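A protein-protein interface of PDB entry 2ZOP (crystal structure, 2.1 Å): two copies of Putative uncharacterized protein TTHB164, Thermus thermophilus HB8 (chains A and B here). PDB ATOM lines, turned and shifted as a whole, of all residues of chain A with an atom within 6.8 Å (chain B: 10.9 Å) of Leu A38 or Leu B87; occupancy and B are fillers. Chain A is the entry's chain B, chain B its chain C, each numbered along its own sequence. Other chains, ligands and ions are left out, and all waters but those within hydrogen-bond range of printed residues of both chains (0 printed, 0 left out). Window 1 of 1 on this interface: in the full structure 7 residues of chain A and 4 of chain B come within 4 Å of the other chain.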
ATOM      1  N   MET A  31      13.062 -15.343 -36.507  1.00  0.00           N
ATOM      2  CA  MET A  31      13.159 -16.041 -35.228  1.00  0.00           C
ATOM      3  C   MET A  31      14.603 -16.233 -34.809  1.00  0.00           C
ATOM      4  O   MET A  31      14.929 -16.146 -33.631  1.00  0.00           O
ATOM      5  CB  MET A  31      12.472 -17.401 -35.310  1.00  0.00           C
ATOM      6  CG  MET A  31      11.085 -17.391 -34.724  1.00  0.00           C
ATOM      7  SD  MET A  31      11.070 -17.650 -32.809  1.00  0.00           S
ATOM      8  CE  MET A  31      11.777 -15.972 -32.177  1.00  0.00           C
ATOM      9  N   LYS A  34      15.784 -13.138 -33.038  1.00  0.00           N
ATOM     10  CA  LYS A  34      15.253 -12.829 -31.709  1.00  0.00           C
ATOM     11  C   LYS A  34      15.569 -13.816 -30.584  1.00  0.00           C
ATOM     12  O   LYS A  34      15.549 -13.442 -29.400  1.00  0.00           O
ATOM     13  CB  LYS A  34      13.733 -12.665 -31.799  1.00  0.00           C
ATOM     14  CG  LYS A  34      13.299 -11.398 -32.503  1.00  0.00           C
ATOM     15  CD  LYS A  34      13.752 -10.193 -31.709  1.00  0.00           C
ATOM     16  CE  LYS A  34      13.008  -8.941 -32.129  1.00  0.00           C
ATOM     17  NZ  LYS A  34      13.139  -7.885 -31.081  1.00  0.00           N
ATOM     18  N   LEU A  35      15.862 -15.064 -30.940  1.00  0.00           N
ATOM     19  CA  LEU A  35      16.120 -16.071 -29.922  1.00  0.00           C
ATOM     20  C   LEU A  35      17.187 -15.719 -28.887  1.00  0.00           C
ATOM     21  O   LEU A  35      16.994 -15.968 -27.699  1.00  0.00           O
ATOM     22  CB  LEU A  35      16.454 -17.425 -30.574  1.00  0.00           C
ATOM     23  CG  LEU A  35      16.476 -18.602 -29.582  1.00  0.00           C
ATOM     24  CD1 LEU A  35      15.197 -18.592 -28.729  1.00  0.00           C
ATOM     25  CD2 LEU A  35      16.589 -19.917 -30.321  1.00  0.00           C
ATOM     26  N   PRO A  36      18.323 -15.135 -29.310  1.00  0.00           N
ATOM     27  CA  PRO A  36      19.337 -14.814 -28.299  1.00  0.00           C
ATOM     28  C   PRO A  36      18.849 -13.883 -27.188  1.00  0.00           C
ATOM     29  O   PRO A  36      18.988 -14.195 -26.000  1.00  0.00           O
ATOM     30  CB  PRO A  36      20.477 -14.200 -29.127  1.00  0.00           C
ATOM     31  CG  PRO A  36      20.322 -14.881 -30.462  1.00  0.00           C
ATOM     32  CD  PRO A  36      18.824 -14.849 -30.665  1.00  0.00           C
ATOM     33  N   VAL A  37      18.260 -12.754 -27.563  1.00  0.00           N
ATOM     34  CA  VAL A  37      17.795 -11.820 -26.549  1.00  0.00           C
ATOM     35  C   VAL A  37      16.689 -12.456 -25.698  1.00  0.00           C
ATOM     36  O   VAL A  37      16.574 -12.169 -24.501  1.00  0.00           O
ATOM     37  CB  VAL A  37      17.336 -10.466 -27.187  1.00  0.00           C
ATOM     38  CG1 VAL A  37      16.060 -10.640 -27.981  1.00  0.00           C
ATOM     39  CG2 VAL A  37      17.166  -9.416 -26.102  1.00  0.00           C
ATOM     40  N   LEU A  38      15.894 -13.337 -26.301  1.00  0.00           N
ATOM     41  CA  LEU A  38      14.846 -14.026 -25.555  1.00  0.00           C
ATOM     42  C   LEU A  38      15.480 -14.860 -24.444  1.00  0.00           C
ATOM     43  O   LEU A  38      15.042 -14.825 -23.296  1.00  0.00           O
ATOM     44  CB  LEU A  38      14.035 -14.941 -26.476  1.00  0.00           C
ATOM     45  CG  LEU A  38      13.055 -14.234 -27.407  1.00  0.00           C
ATOM     46  CD1 LEU A  38      12.387 -15.240 -28.308  1.00  0.00           C
ATOM     47  CD2 LEU A  38      12.026 -13.488 -26.569  1.00  0.00           C
ATOM     48  N   VAL A  39      16.509 -15.623 -24.793  1.00  0.00           N
ATOM     49  CA  VAL A  39      17.198 -16.452 -23.810  1.00  0.00           C
ATOM     50  C   VAL A  39      17.884 -15.591 -22.750  1.00  0.00           C
ATOM     51  O   VAL A  39      17.774 -15.870 -21.558  1.00  0.00           O
ATOM     52  CB  VAL A  39      18.239 -17.377 -24.495  1.00  0.00           C
ATOM     53  CG1 VAL A  39      19.055 -18.118 -23.459  1.00  0.00           C
ATOM     54  CG2 VAL A  39      17.521 -18.382 -25.390  1.00  0.00           C
ATOM     55  N   ARG A  40      18.577 -14.539 -23.176  1.00  0.00           N
ATOM     56  CA  ARG A  40      19.270 -13.653 -22.238  1.00  0.00           C
ATOM     57  C   ARG A  40      18.350 -12.915 -21.254  1.00  0.00           C
ATOM     58  O   ARG A  40      18.599 -12.910 -20.046  1.00  0.00           O
ATOM     59  CB  ARG A  40      20.086 -12.597 -22.988  1.00  0.00           C
ATOM     60  CG  ARG A  40      21.381 -13.088 -23.611  1.00  0.00           C
ATOM     61  CD  ARG A  40      22.272 -11.889 -23.931  1.00  0.00           C
ATOM     62  NE  ARG A  40      21.622 -10.975 -24.870  1.00  0.00           N
ATOM     63  CZ  ARG A  40      21.727 -11.070 -26.190  1.00  0.00           C
ATOM     64  NH1 ARG A  40      22.463 -12.038 -26.729  1.00  0.00           N
ATOM     65  NH2 ARG A  40      21.095 -10.208 -26.973  1.00  0.00           N
ATOM     66  N   GLN A  41      17.297 -12.292 -21.780  1.00  0.00           N
ATOM     67  CA  GLN A  41      16.364 -11.508 -20.968  1.00  0.00           C
ATOM     68  C   GLN A  41      15.250 -12.299 -20.283  1.00  0.00           C
ATOM     69  O   GLN A  41      14.911 -12.015 -19.142  1.00  0.00           O
ATOM     70  CB  GLN A  41      15.711 -10.417 -21.825  1.00  0.00           C
ATOM     71  CG  GLN A  41      16.623  -9.762 -22.844  1.00  0.00           C
ATOM     72  CD  GLN A  41      17.592  -8.770 -22.243  1.00  0.00           C
ATOM     73  OE1 GLN A  41      18.289  -9.072 -21.270  1.00  0.00           O
ATOM     74  NE2 GLN A  41      17.653  -7.573 -22.832  1.00  0.00           N
ATOM     75  N   ALA A  42      14.671 -13.277 -20.971  1.00  0.00           N
ATOM     76  CA  ALA A  42      13.571 -14.054 -20.388  1.00  0.00           C
ATOM     77  C   ALA A  42      13.941 -15.394 -19.747  1.00  0.00           C
ATOM     78  O   ALA A  42      13.138 -15.968 -19.006  1.00  0.00           O
ATOM     79  CB  ALA A  42      12.490 -14.279 -21.436  1.00  0.00           C
ATOM     80  N   GLY A  43      15.137 -15.902 -20.027  1.00  0.00           N
ATOM     81  CA  GLY A  43      15.531 -17.183 -19.455  1.00  0.00           C
ATOM     82  C   GLY A  43      15.299 -18.309 -20.453  1.00  0.00           C
ATOM     83  O   GLY A  43      14.453 -18.176 -21.336  1.00  0.00           O
ATOM     84  N   LEU A  44      16.028 -19.417 -20.314  1.00  0.00           N
ATOM     85  CA  LEU A  44      15.899 -20.540 -21.247  1.00  0.00           C
ATOM     86  C   LEU A  44      14.500 -21.134 -21.361  1.00  0.00           C
ATOM     87  O   LEU A  44      13.951 -21.245 -22.465  1.00  0.00           O
ATOM     88  CB  LEU A  44      16.897 -21.654 -20.881  1.00  0.00           C
ATOM     89  CG  LEU A  44      16.834 -22.958 -21.706  1.00  0.00           C
ATOM     90  CD1 LEU A  44      17.211 -22.690 -23.175  1.00  0.00           C
ATOM     91  CD2 LEU A  44      17.795 -23.962 -21.113  1.00  0.00           C
ATOM     92  N   GLN A  46      11.493 -19.990 -20.627  1.00  0.00           N
ATOM     93  CA  GLN A  46      10.524 -19.122 -21.279  1.00  0.00           C
ATOM     94  C   GLN A  46      10.834 -18.977 -22.763  1.00  0.00           C
ATOM     95  O   GLN A  46       9.939 -19.064 -23.594  1.00  0.00           O
ATOM     96  CB  GLN A  46      10.493 -17.741 -20.622  1.00  0.00           C
ATOM     97  CG  GLN A  46      10.152 -17.768 -19.145  1.00  0.00           C
ATOM     98  CD  GLN A  46       9.792 -16.396 -18.608  1.00  0.00           C
ATOM     99  OE1 GLN A  46       9.920 -16.134 -17.408  1.00  0.00           O
ATOM    100  NE2 GLN A  46       9.324 -15.516 -19.493  1.00  0.00           N
ATOM    101  N   ALA A  47      12.105 -18.761 -23.094  1.00  0.00           N
ATOM    102  CA  ALA A  47      12.491 -18.615 -24.493  1.00  0.00           C
ATOM    103  C   ALA A  47      12.052 -19.824 -25.319  1.00  0.00           C
ATOM    104  O   ALA A  47      11.477 -19.663 -26.401  1.00  0.00           O
ATOM    105  CB  ALA A  47      13.990 -18.421 -24.607  1.00  0.00           C
ATOM    106  N   LEU A  48      12.314 -21.030 -24.809  1.00  0.00           N
ATOM    107  CA  LEU A  48      11.938 -22.245 -25.529  1.00  0.00           C
ATOM    108  C   LEU A  48      10.425 -22.415 -25.611  1.00  0.00           C
ATOM    109  O   LEU A  48       9.907 -22.896 -26.617  1.00  0.00           O
ATOM    110  CB  LEU A  48      12.545 -23.490 -24.870  1.00  0.00           C
ATOM    111  CG  LEU A  48      14.077 -23.575 -24.789  1.00  0.00           C
ATOM    112  CD1 LEU A  48      14.490 -24.926 -24.205  1.00  0.00           C
ATOM    113  CD2 LEU A  48      14.677 -23.380 -26.173  1.00  0.00           C
ATOM    114  N   ALA A  49       9.717 -22.044 -24.547  1.00  0.00           N
ATOM    115  CA  ALA A  49       8.264 -22.175 -24.540  1.00  0.00           C
ATOM    116  C   ALA A  49       7.682 -21.227 -25.585  1.00  0.00           C
ATOM    117  O   ALA A  49       6.708 -21.551 -26.253  1.00  0.00           O
ATOM    118  CB  ALA A  49       7.708 -21.854 -23.159  1.00  0.00           C
ATOM    119  N   PHE A  50       8.292 -20.054 -25.731  1.00  0.00           N
ATOM    120  CA  PHE A  50       7.820 -19.091 -26.718  1.00  0.00           C
ATOM    121  C   PHE A  50       7.971 -19.658 -28.126  1.00  0.00           C
ATOM    122  O   PHE A  50       7.038 -19.628 -28.932  1.00  0.00           O
ATOM    123  CB  PHE A  50       8.616 -17.793 -26.631  1.00  0.00           C
ATOM    124  CG  PHE A  50       8.191 -16.766 -27.640  1.00  0.00           C
ATOM    125  CD1 PHE A  50       6.981 -16.093 -27.496  1.00  0.00           C
ATOM    126  CD2 PHE A  50       8.988 -16.486 -28.744  1.00  0.00           C
ATOM    127  CE1 PHE A  50       6.574 -15.153 -28.437  1.00  0.00           C
ATOM    128  CE2 PHE A  50       8.587 -15.548 -29.691  1.00  0.00           C
ATOM    129  CZ  PHE A  50       7.375 -14.878 -29.538  1.00  0.00           C
ATOM    130  N   VAL A  51       9.157 -20.178 -28.417  1.00  0.00           N
ATOM    131  CA  VAL A  51       9.415 -20.734 -29.733  1.00  0.00           C
ATOM    132  C   VAL A  51       8.512 -21.923 -30.031  1.00  0.00           C
ATOM    133  O   VAL A  51       7.987 -22.045 -31.137  1.00  0.00           O
ATOM    134  CB  VAL A  51      10.887 -21.171 -29.883  1.00  0.00           C
ATOM    135  CG1 VAL A  51      11.083 -21.853 -31.224  1.00  0.00           C
ATOM    136  CG2 VAL A  51      11.806 -19.953 -29.791  1.00  0.00           C
ATOM    137  N   ARG A  54       4.848 -20.998 -31.100  1.00  0.00           N
ATOM    138  CA  ARG A  54       4.627 -20.171 -32.284  1.00  0.00           C
ATOM    139  C   ARG A  54       3.793 -20.917 -33.320  1.00  0.00           C
ATOM    140  O   ARG A  54       3.948 -22.123 -33.501  1.00  0.00           O
ATOM    141  CB  ARG A  54       5.957 -19.739 -32.913  1.00  0.00           C
ATOM    142  CG  ARG A  54       6.830 -18.831 -32.043  1.00  0.00           C
ATOM    143  CD  ARG A  54       6.073 -17.629 -31.488  1.00  0.00           C
ATOM    144  NE  ARG A  54       5.301 -17.984 -30.302  1.00  0.00           N
ATOM    145  CZ  ARG A  54       4.436 -17.181 -29.689  1.00  0.00           C
ATOM    146  NH1 ARG A  54       4.215 -15.957 -30.144  1.00  0.00           N
ATOM    147  NH2 ARG A  54       3.791 -17.606 -28.612  1.00  0.00           N
ATOM    148  N   GLY B  43      12.497  -7.149 -12.659  1.00  0.00           N
ATOM    149  CA  GLY B  43      11.661  -7.350 -13.836  1.00  0.00           C
ATOM    150  C   GLY B  43      10.553  -6.310 -13.856  1.00  0.00           C
ATOM    151  O   GLY B  43      10.196  -5.780 -12.809  1.00  0.00           O
ATOM    152  N   LEU B  44       9.993  -6.016 -15.028  1.00  0.00           N
ATOM    153  CA  LEU B  44       8.948  -4.993 -15.125  1.00  0.00           C
ATOM    154  C   LEU B  44       7.711  -5.191 -14.243  1.00  0.00           C
ATOM    155  O   LEU B  44       7.376  -4.320 -13.445  1.00  0.00           O
ATOM    156  CB  LEU B  44       8.505  -4.818 -16.587  1.00  0.00           C
ATOM    157  CG  LEU B  44       7.436  -3.743 -16.848  1.00  0.00           C
ATOM    158  CD1 LEU B  44       7.903  -2.387 -16.317  1.00  0.00           C
ATOM    159  CD2 LEU B  44       7.151  -3.661 -18.346  1.00  0.00           C
ATOM    160  N   SER B  45       7.027  -6.320 -14.375  1.00  0.00           N
ATOM    161  CA  SER B  45       5.820  -6.540 -13.576  1.00  0.00           C
ATOM    162  C   SER B  45       6.021  -6.447 -12.057  1.00  0.00           C
ATOM    163  O   SER B  45       5.216  -5.817 -11.374  1.00  0.00           O
ATOM    164  CB  SER B  45       5.174  -7.874 -13.943  1.00  0.00           C
ATOM    165  OG  SER B  45       4.707  -7.835 -15.279  1.00  0.00           O
ATOM    166  N   ALA B  81      -0.977  -3.940 -19.085  1.00  0.00           N
ATOM    167  CA  ALA B  81      -0.366  -4.160 -20.391  1.00  0.00           C
ATOM    168  C   ALA B  81       0.858  -5.068 -20.309  1.00  0.00           C
ATOM    169  O   ALA B  81       1.073  -5.905 -21.177  1.00  0.00           O
ATOM    170  CB  ALA B  81       0.025  -2.817 -21.022  1.00  0.00           C
ATOM    171  N   ALA B  82       1.667  -4.893 -19.269  1.00  0.00           N
ATOM    172  CA  ALA B  82       2.869  -5.709 -19.109  1.00  0.00           C
ATOM    173  C   ALA B  82       2.492  -7.163 -18.849  1.00  0.00           C
ATOM    174  O   ALA B  82       3.119  -8.067 -19.370  1.00  0.00           O
ATOM    175  CB  ALA B  82       3.728  -5.179 -17.965  1.00  0.00           C
ATOM    176  N   ARG B  83       1.458  -7.388 -18.048  1.00  0.00           N
ATOM    177  CA  ARG B  83       1.048  -8.762 -17.758  1.00  0.00           C
ATOM    178  C   ARG B  83       0.358  -9.435 -18.948  1.00  0.00           C
ATOM    179  O   ARG B  83       0.470 -10.650 -19.136  1.00  0.00           O
ATOM    180  CB  ARG B  83       0.121  -8.809 -16.541  1.00  0.00           C
ATOM    181  CG  ARG B  83       0.810  -8.530 -15.212  1.00  0.00           C
ATOM    182  CD  ARG B  83      -0.128  -8.845 -14.045  1.00  0.00           C
ATOM    183  NE  ARG B  83      -1.346  -8.043 -14.094  1.00  0.00           N
ATOM    184  CZ  ARG B  83      -1.521  -6.899 -13.430  1.00  0.00           C
ATOM    185  NH1 ARG B  83      -2.664  -6.232 -13.539  1.00  0.00           N
ATOM    186  NH2 ARG B  83      -0.554  -6.425 -12.655  1.00  0.00           N
ATOM    187  N   GLU B  84      -0.337  -8.647 -19.762  1.00  0.00           N
ATOM    188  CA  GLU B  84      -1.043  -9.194 -20.921  1.00  0.00           C
ATOM    189  C   GLU B  84      -0.132  -9.428 -22.126  1.00  0.00           C
ATOM    190  O   GLU B  84      -0.405 -10.287 -22.969  1.00  0.00           O
ATOM    191  CB  GLU B  84      -2.182  -8.250 -21.330  1.00  0.00           C
ATOM    192  CG  GLU B  84      -3.256  -8.063 -20.261  1.00  0.00           C
ATOM    193  CD  GLU B  84      -4.247  -6.958 -20.602  1.00  0.00           C
ATOM    194  OE1 GLU B  84      -5.204  -6.769 -19.829  1.00  0.00           O
ATOM    195  OE2 GLU B  84      -4.069  -6.275 -21.631  1.00  0.00           O
ATOM    196  N   ALA B  85       0.954  -8.667 -22.200  1.00  0.00           N
ATOM    197  CA  ALA B  85       1.889  -8.760 -23.314  1.00  0.00           C
ATOM    198  C   ALA B  85       2.528 -10.127 -23.553  1.00  0.00           C
ATOM    199  O   ALA B  85       2.829 -10.863 -22.610  1.00  0.00           O
ATOM    200  CB  ALA B  85       2.987  -7.716 -23.138  1.00  0.00           C
ATOM    201  N   GLU B  86       2.727 -10.464 -24.827  1.00  0.00           N
ATOM    202  CA  GLU B  86       3.402 -11.709 -25.169  1.00  0.00           C
ATOM    203  C   GLU B  86       4.867 -11.399 -24.888  1.00  0.00           C
ATOM    204  O   GLU B  86       5.241 -10.230 -24.818  1.00  0.00           O
ATOM    205  CB  GLU B  86       3.200 -12.074 -26.640  1.00  0.00           C
ATOM    206  CG  GLU B  86       1.789 -12.552 -26.954  1.00  0.00           C
ATOM    207  CD  GLU B  86       1.720 -13.399 -28.210  1.00  0.00           C
ATOM    208  OE1 GLU B  86       2.042 -12.886 -29.307  1.00  0.00           O
ATOM    209  OE2 GLU B  86       1.339 -14.584 -28.092  1.00  0.00           O
ATOM    210  N   LEU B  87       5.685 -12.434 -24.742  1.00  0.00           N
ATOM    211  CA  LEU B  87       7.093 -12.269 -24.410  1.00  0.00           C
ATOM    212  C   LEU B  87       7.876 -11.175 -25.143  1.00  0.00           C
ATOM    213  O   LEU B  87       8.547 -10.379 -24.500  1.00  0.00           O
ATOM    214  CB  LEU B  87       7.815 -13.615 -24.542  1.00  0.00           C
ATOM    215  CG  LEU B  87       9.218 -13.687 -23.924  1.00  0.00           C
ATOM    216  CD1 LEU B  87       9.182 -13.190 -22.475  1.00  0.00           C
ATOM    217  CD2 LEU B  87       9.731 -15.122 -23.984  1.00  0.00           C
ATOM    218  N   LEU B  88       7.796 -11.121 -26.468  1.00  0.00           N
ATOM    219  CA  LEU B  88       8.531 -10.096 -27.220  1.00  0.00           C
ATOM    220  C   LEU B  88       8.069  -8.676 -26.896  1.00  0.00           C
ATOM    221  O   LEU B  88       8.885  -7.764 -26.753  1.00  0.00           O
ATOM    222  CB  LEU B  88       8.413 -10.339 -28.731  1.00  0.00           C
ATOM    223  CG  LEU B  88       9.471 -11.243 -29.372  1.00  0.00           C
ATOM    224  CD1 LEU B  88      10.829 -10.555 -29.351  1.00  0.00           C
ATOM    225  CD2 LEU B  88       9.533 -12.559 -28.631  1.00  0.00           C
ATOM    226  N   GLN B  89       6.762  -8.484 -26.779  1.00  0.00           N
ATOM    227  CA  GLN B  89       6.242  -7.168 -26.458  1.00  0.00           C
ATOM    228  C   GLN B  89       6.582  -6.817 -25.011  1.00  0.00           C
ATOM    229  O   GLN B  89       6.735  -5.645 -24.674  1.00  0.00           O
ATOM    230  CB  GLN B  89       4.724  -7.122 -26.684  1.00  0.00           C
ATOM    231  CG  GLN B  89       4.099  -5.748 -26.486  1.00  0.00           C
ATOM    232  CD  GLN B  89       4.875  -4.639 -27.195  1.00  0.00           C
ATOM    233  OE1 GLN B  89       5.322  -4.802 -28.335  1.00  0.00           O
ATOM    234  NE2 GLN B  89       5.029  -3.501 -26.520  1.00  0.00           N
ATOM    235  N   TYR B  90       6.712  -7.836 -24.161  1.00  0.00           N
ATOM    236  CA  TYR B  90       7.043  -7.608 -22.754  1.00  0.00           C
ATOM    237  C   TYR B  90       8.447  -7.032 -22.657  1.00  0.00           C
ATOM    238  O   TYR B  90       8.681  -6.068 -21.928  1.00  0.00           O
ATOM    239  CB  TYR B  90       6.977  -8.913 -21.955  1.00  0.00           C
ATOM    240  CG  TYR B  90       7.246  -8.740 -20.477  1.00  0.00           C
ATOM    241  CD1 TYR B  90       6.311  -8.115 -19.650  1.00  0.00           C
ATOM    242  CD2 TYR B  90       8.438  -9.199 -19.900  1.00  0.00           C
ATOM    243  CE1 TYR B  90       6.549  -7.956 -18.284  1.00  0.00           C
ATOM    244  CE2 TYR B  90       8.688  -9.041 -18.529  1.00  0.00           C
ATOM    245  CZ  TYR B  90       7.736  -8.420 -17.729  1.00  0.00           C
ATOM    246  OH  TYR B  90       7.951  -8.266 -16.377  1.00  0.00           O
ATOM    247  N   LEU B  91       9.384  -7.623 -23.396  1.00  0.00           N
ATOM    248  CA  LEU B  91      10.762  -7.138 -23.378  1.00  0.00           C
ATOM    249  C   LEU B  91      10.842  -5.734 -23.974  1.00  0.00           C
ATOM    250  O   LEU B  91      11.621  -4.908 -23.515  1.00  0.00           O
ATOM    251  CB  LEU B  91      11.683  -8.100 -24.145  1.00  0.00           C
ATOM    252  CG  LEU B  91      11.761  -9.520 -23.562  1.00  0.00           C
ATOM    253  CD1 LEU B  91      12.790 -10.338 -24.323  1.00  0.00           C
ATOM    254  CD2 LEU B  91      12.132  -9.460 -22.082  1.00  0.00           C
ATOM    255  N   ARG B  92      10.027  -5.462 -24.991  1.00  0.00           N
ATOM    256  CA  ARG B  92      10.008  -4.141 -25.617  1.00  0.00           C
ATOM    257  C   ARG B  92       9.496  -3.112 -24.608  1.00  0.00           C
ATOM    258  O   ARG B  92      10.066  -2.032 -24.444  1.00  0.00           O
ATOM    259  CB  ARG B  92       9.103  -4.152 -26.859  1.00  0.00           C
ATOM    260  CG  ARG B  92       9.112  -2.852 -27.657  1.00  0.00           C
ATOM    261  CD  ARG B  92       8.221  -2.939 -28.900  1.00  0.00           C
ATOM    262  NE  ARG B  92       8.403  -1.789 -29.788  1.00  0.00           N
ATOM    263  CZ  ARG B  92       7.771  -1.627 -30.949  1.00  0.00           C
ATOM    264  NH1 ARG B  92       6.906  -2.540 -31.375  1.00  0.00           N
ATOM    265  NH2 ARG B  92       8.005  -0.549 -31.689  1.00  0.00           N
ATOM    266  N   LEU B  93       8.416  -3.462 -23.926  1.00  0.00           N
ATOM    267  CA  LEU B  93       7.832  -2.579 -22.926  1.00  0.00           C
ATOM    268  C   LEU B  93       8.824  -2.305 -21.789  1.00  0.00           C
ATOM    269  O   LEU B  93       8.897  -1.191 -21.273  1.00  0.00           O
ATOM    270  CB  LEU B  93       6.561  -3.210 -22.374  1.00  0.00           C
ATOM    271  CG  LEU B  93       5.748  -2.377 -21.385  1.00  0.00           C
ATOM    272  CD1 LEU B  93       5.358  -1.025 -22.000  1.00  0.00           C
ATOM    273  CD2 LEU B  93       4.516  -3.170 -21.001  1.00  0.00           C
ATOM    274  N   THR B  94       9.589  -3.324 -21.415  1.00  0.00           N
ATOM    275  CA  THR B  94      10.581  -3.195 -20.349  1.00  0.00           C
ATOM    276  C   THR B  94      11.634  -2.156 -20.758  1.00  0.00           C
ATOM    277  O   THR B  94      12.001  -1.276 -19.976  1.00  0.00           O
ATOM    278  CB  THR B  94      11.281  -4.558 -20.085  1.00  0.00           C
ATOM    279  OG1 THR B  94      10.341  -5.474 -19.510  1.00  0.00           O
ATOM    280  CG2 THR B  94      12.470  -4.397 -19.146  1.00  0.00           C
ATOM    281  N   ARG B  95      12.115  -2.286 -21.989  1.00  0.00           N
ATOM    282  CA  ARG B  95      13.119  -1.385 -22.551  1.00  0.00           C
ATOM    283  C   ARG B  95      12.572   0.040 -22.557  1.00  0.00           C
ATOM    284  O   ARG B  95      13.263   0.996 -22.197  1.00  0.00           O
ATOM    285  CB  ARG B  95      13.436  -1.823 -23.983  1.00  0.00           C
ATOM    286  CG  ARG B  95      14.523  -1.034 -24.680  1.00  0.00           C
ATOM    287  CD  ARG B  95      14.450  -1.268 -26.180  1.00  0.00           C
ATOM    288  NE  ARG B  95      14.153  -2.666 -26.486  1.00  0.00           N
ATOM    289  CZ  ARG B  95      13.830  -3.118 -27.694  1.00  0.00           C
ATOM    290  NH1 ARG B  95      13.763  -2.283 -28.724  1.00  0.00           N
ATOM    291  NH2 ARG B  95      13.559  -4.406 -27.868  1.00  0.00           N
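Positions printed for both chains: 43 and 44.
Among the printed residues, merely in contact across the chains: Lys A34 with Leu B88, Leu A38 with Leu B87, Leu A38 with Leu B88, Leu A38 with Leu B91, Gln A41 with Leu B91, Ala A42 with Leu B87, Gln A46 with Leu B87, Phe A50 with Leu B87 and Phe A50 with Leu B88.
Of the 18 printed residues of chain B, 4 touch a printed residue of chain A. Hydrophobic or aromatic side chains of chain B within 4 Å of the printed part of chain A: Leu B87, Leu B88 and Leu B91. Of the 19 printed residues of chain A, 7 touch a printed residue of chain B. Hydrophobic or aromatic side chains of chain A within 4 Å of the printed part of chain B: Leu A38, Ala A42 and Phe A50. Among the printed residues, 10 pairs touch across the chains. Among the printed residues, Asp or Glu carboxylates within 4 Å of a Lys or Arg side-chain nitrogen of the other chain: Arg A54 with Glu B86 (3.8 Å).
The guanidinium group (NH1) of Arg A54 is in salt-bridge range of the side-chain carboxylate (OE2) of Glu B86 (3.8 Å).
The backbone NH of Gly A43 sits at hydrogen-bond distance from the backbone carbonyl oxygen of Leu A38, 3.4 Å away. The guanidinium group (NE) of Arg A54 lies within hydrogen-bond range of the backbone carbonyl oxygen (O) of Phe A50 (2.8 Å).
Of the printed residues of chain B, Lys A34 touches Leu B88. No residue of chain B comes within 4 Å of Pro A36. Leu A38 touches just these residues of chain B: Leu B87, Leu B88 and Leu B91. Printed residues of chain B within 4 Å of Gln A41: Leu B91 (3.7 Å). Of the printed residues of chain B, Ala A42 touches Leu B87 (3.6 Å). No residue of chain B comes within 4 Å of Gly A43. Gln A46 touches just one residue of chain B: Leu B87 (3.8 Å). No residue of chain B comes within 4 Å of Ala A47. Of the printed residues of chain B, Phe A50 touches Leu B87 (3.9 Å) and Leu B88 (3.3 Å). Val A51 touches none of the printed residues of chain B. Of the printed residues of chain A, Glu B86 touches Arg A54 (3.8 Å). Of chain A, only Leu A38 (3.8 Å), Ala A42 (3.6 Å), Gln A46 (3.8 Å) and Phe A50 (3.9 Å) come within 4 Å of Leu B87. Printed residues of chain A within 4 Å of Leu B91: Leu A38 (3.9 Å) and Gln A41 (3.7 Å). The nearest printed residue of chain A that does not touch Leu B91 is Val A37 (4.2 Å).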
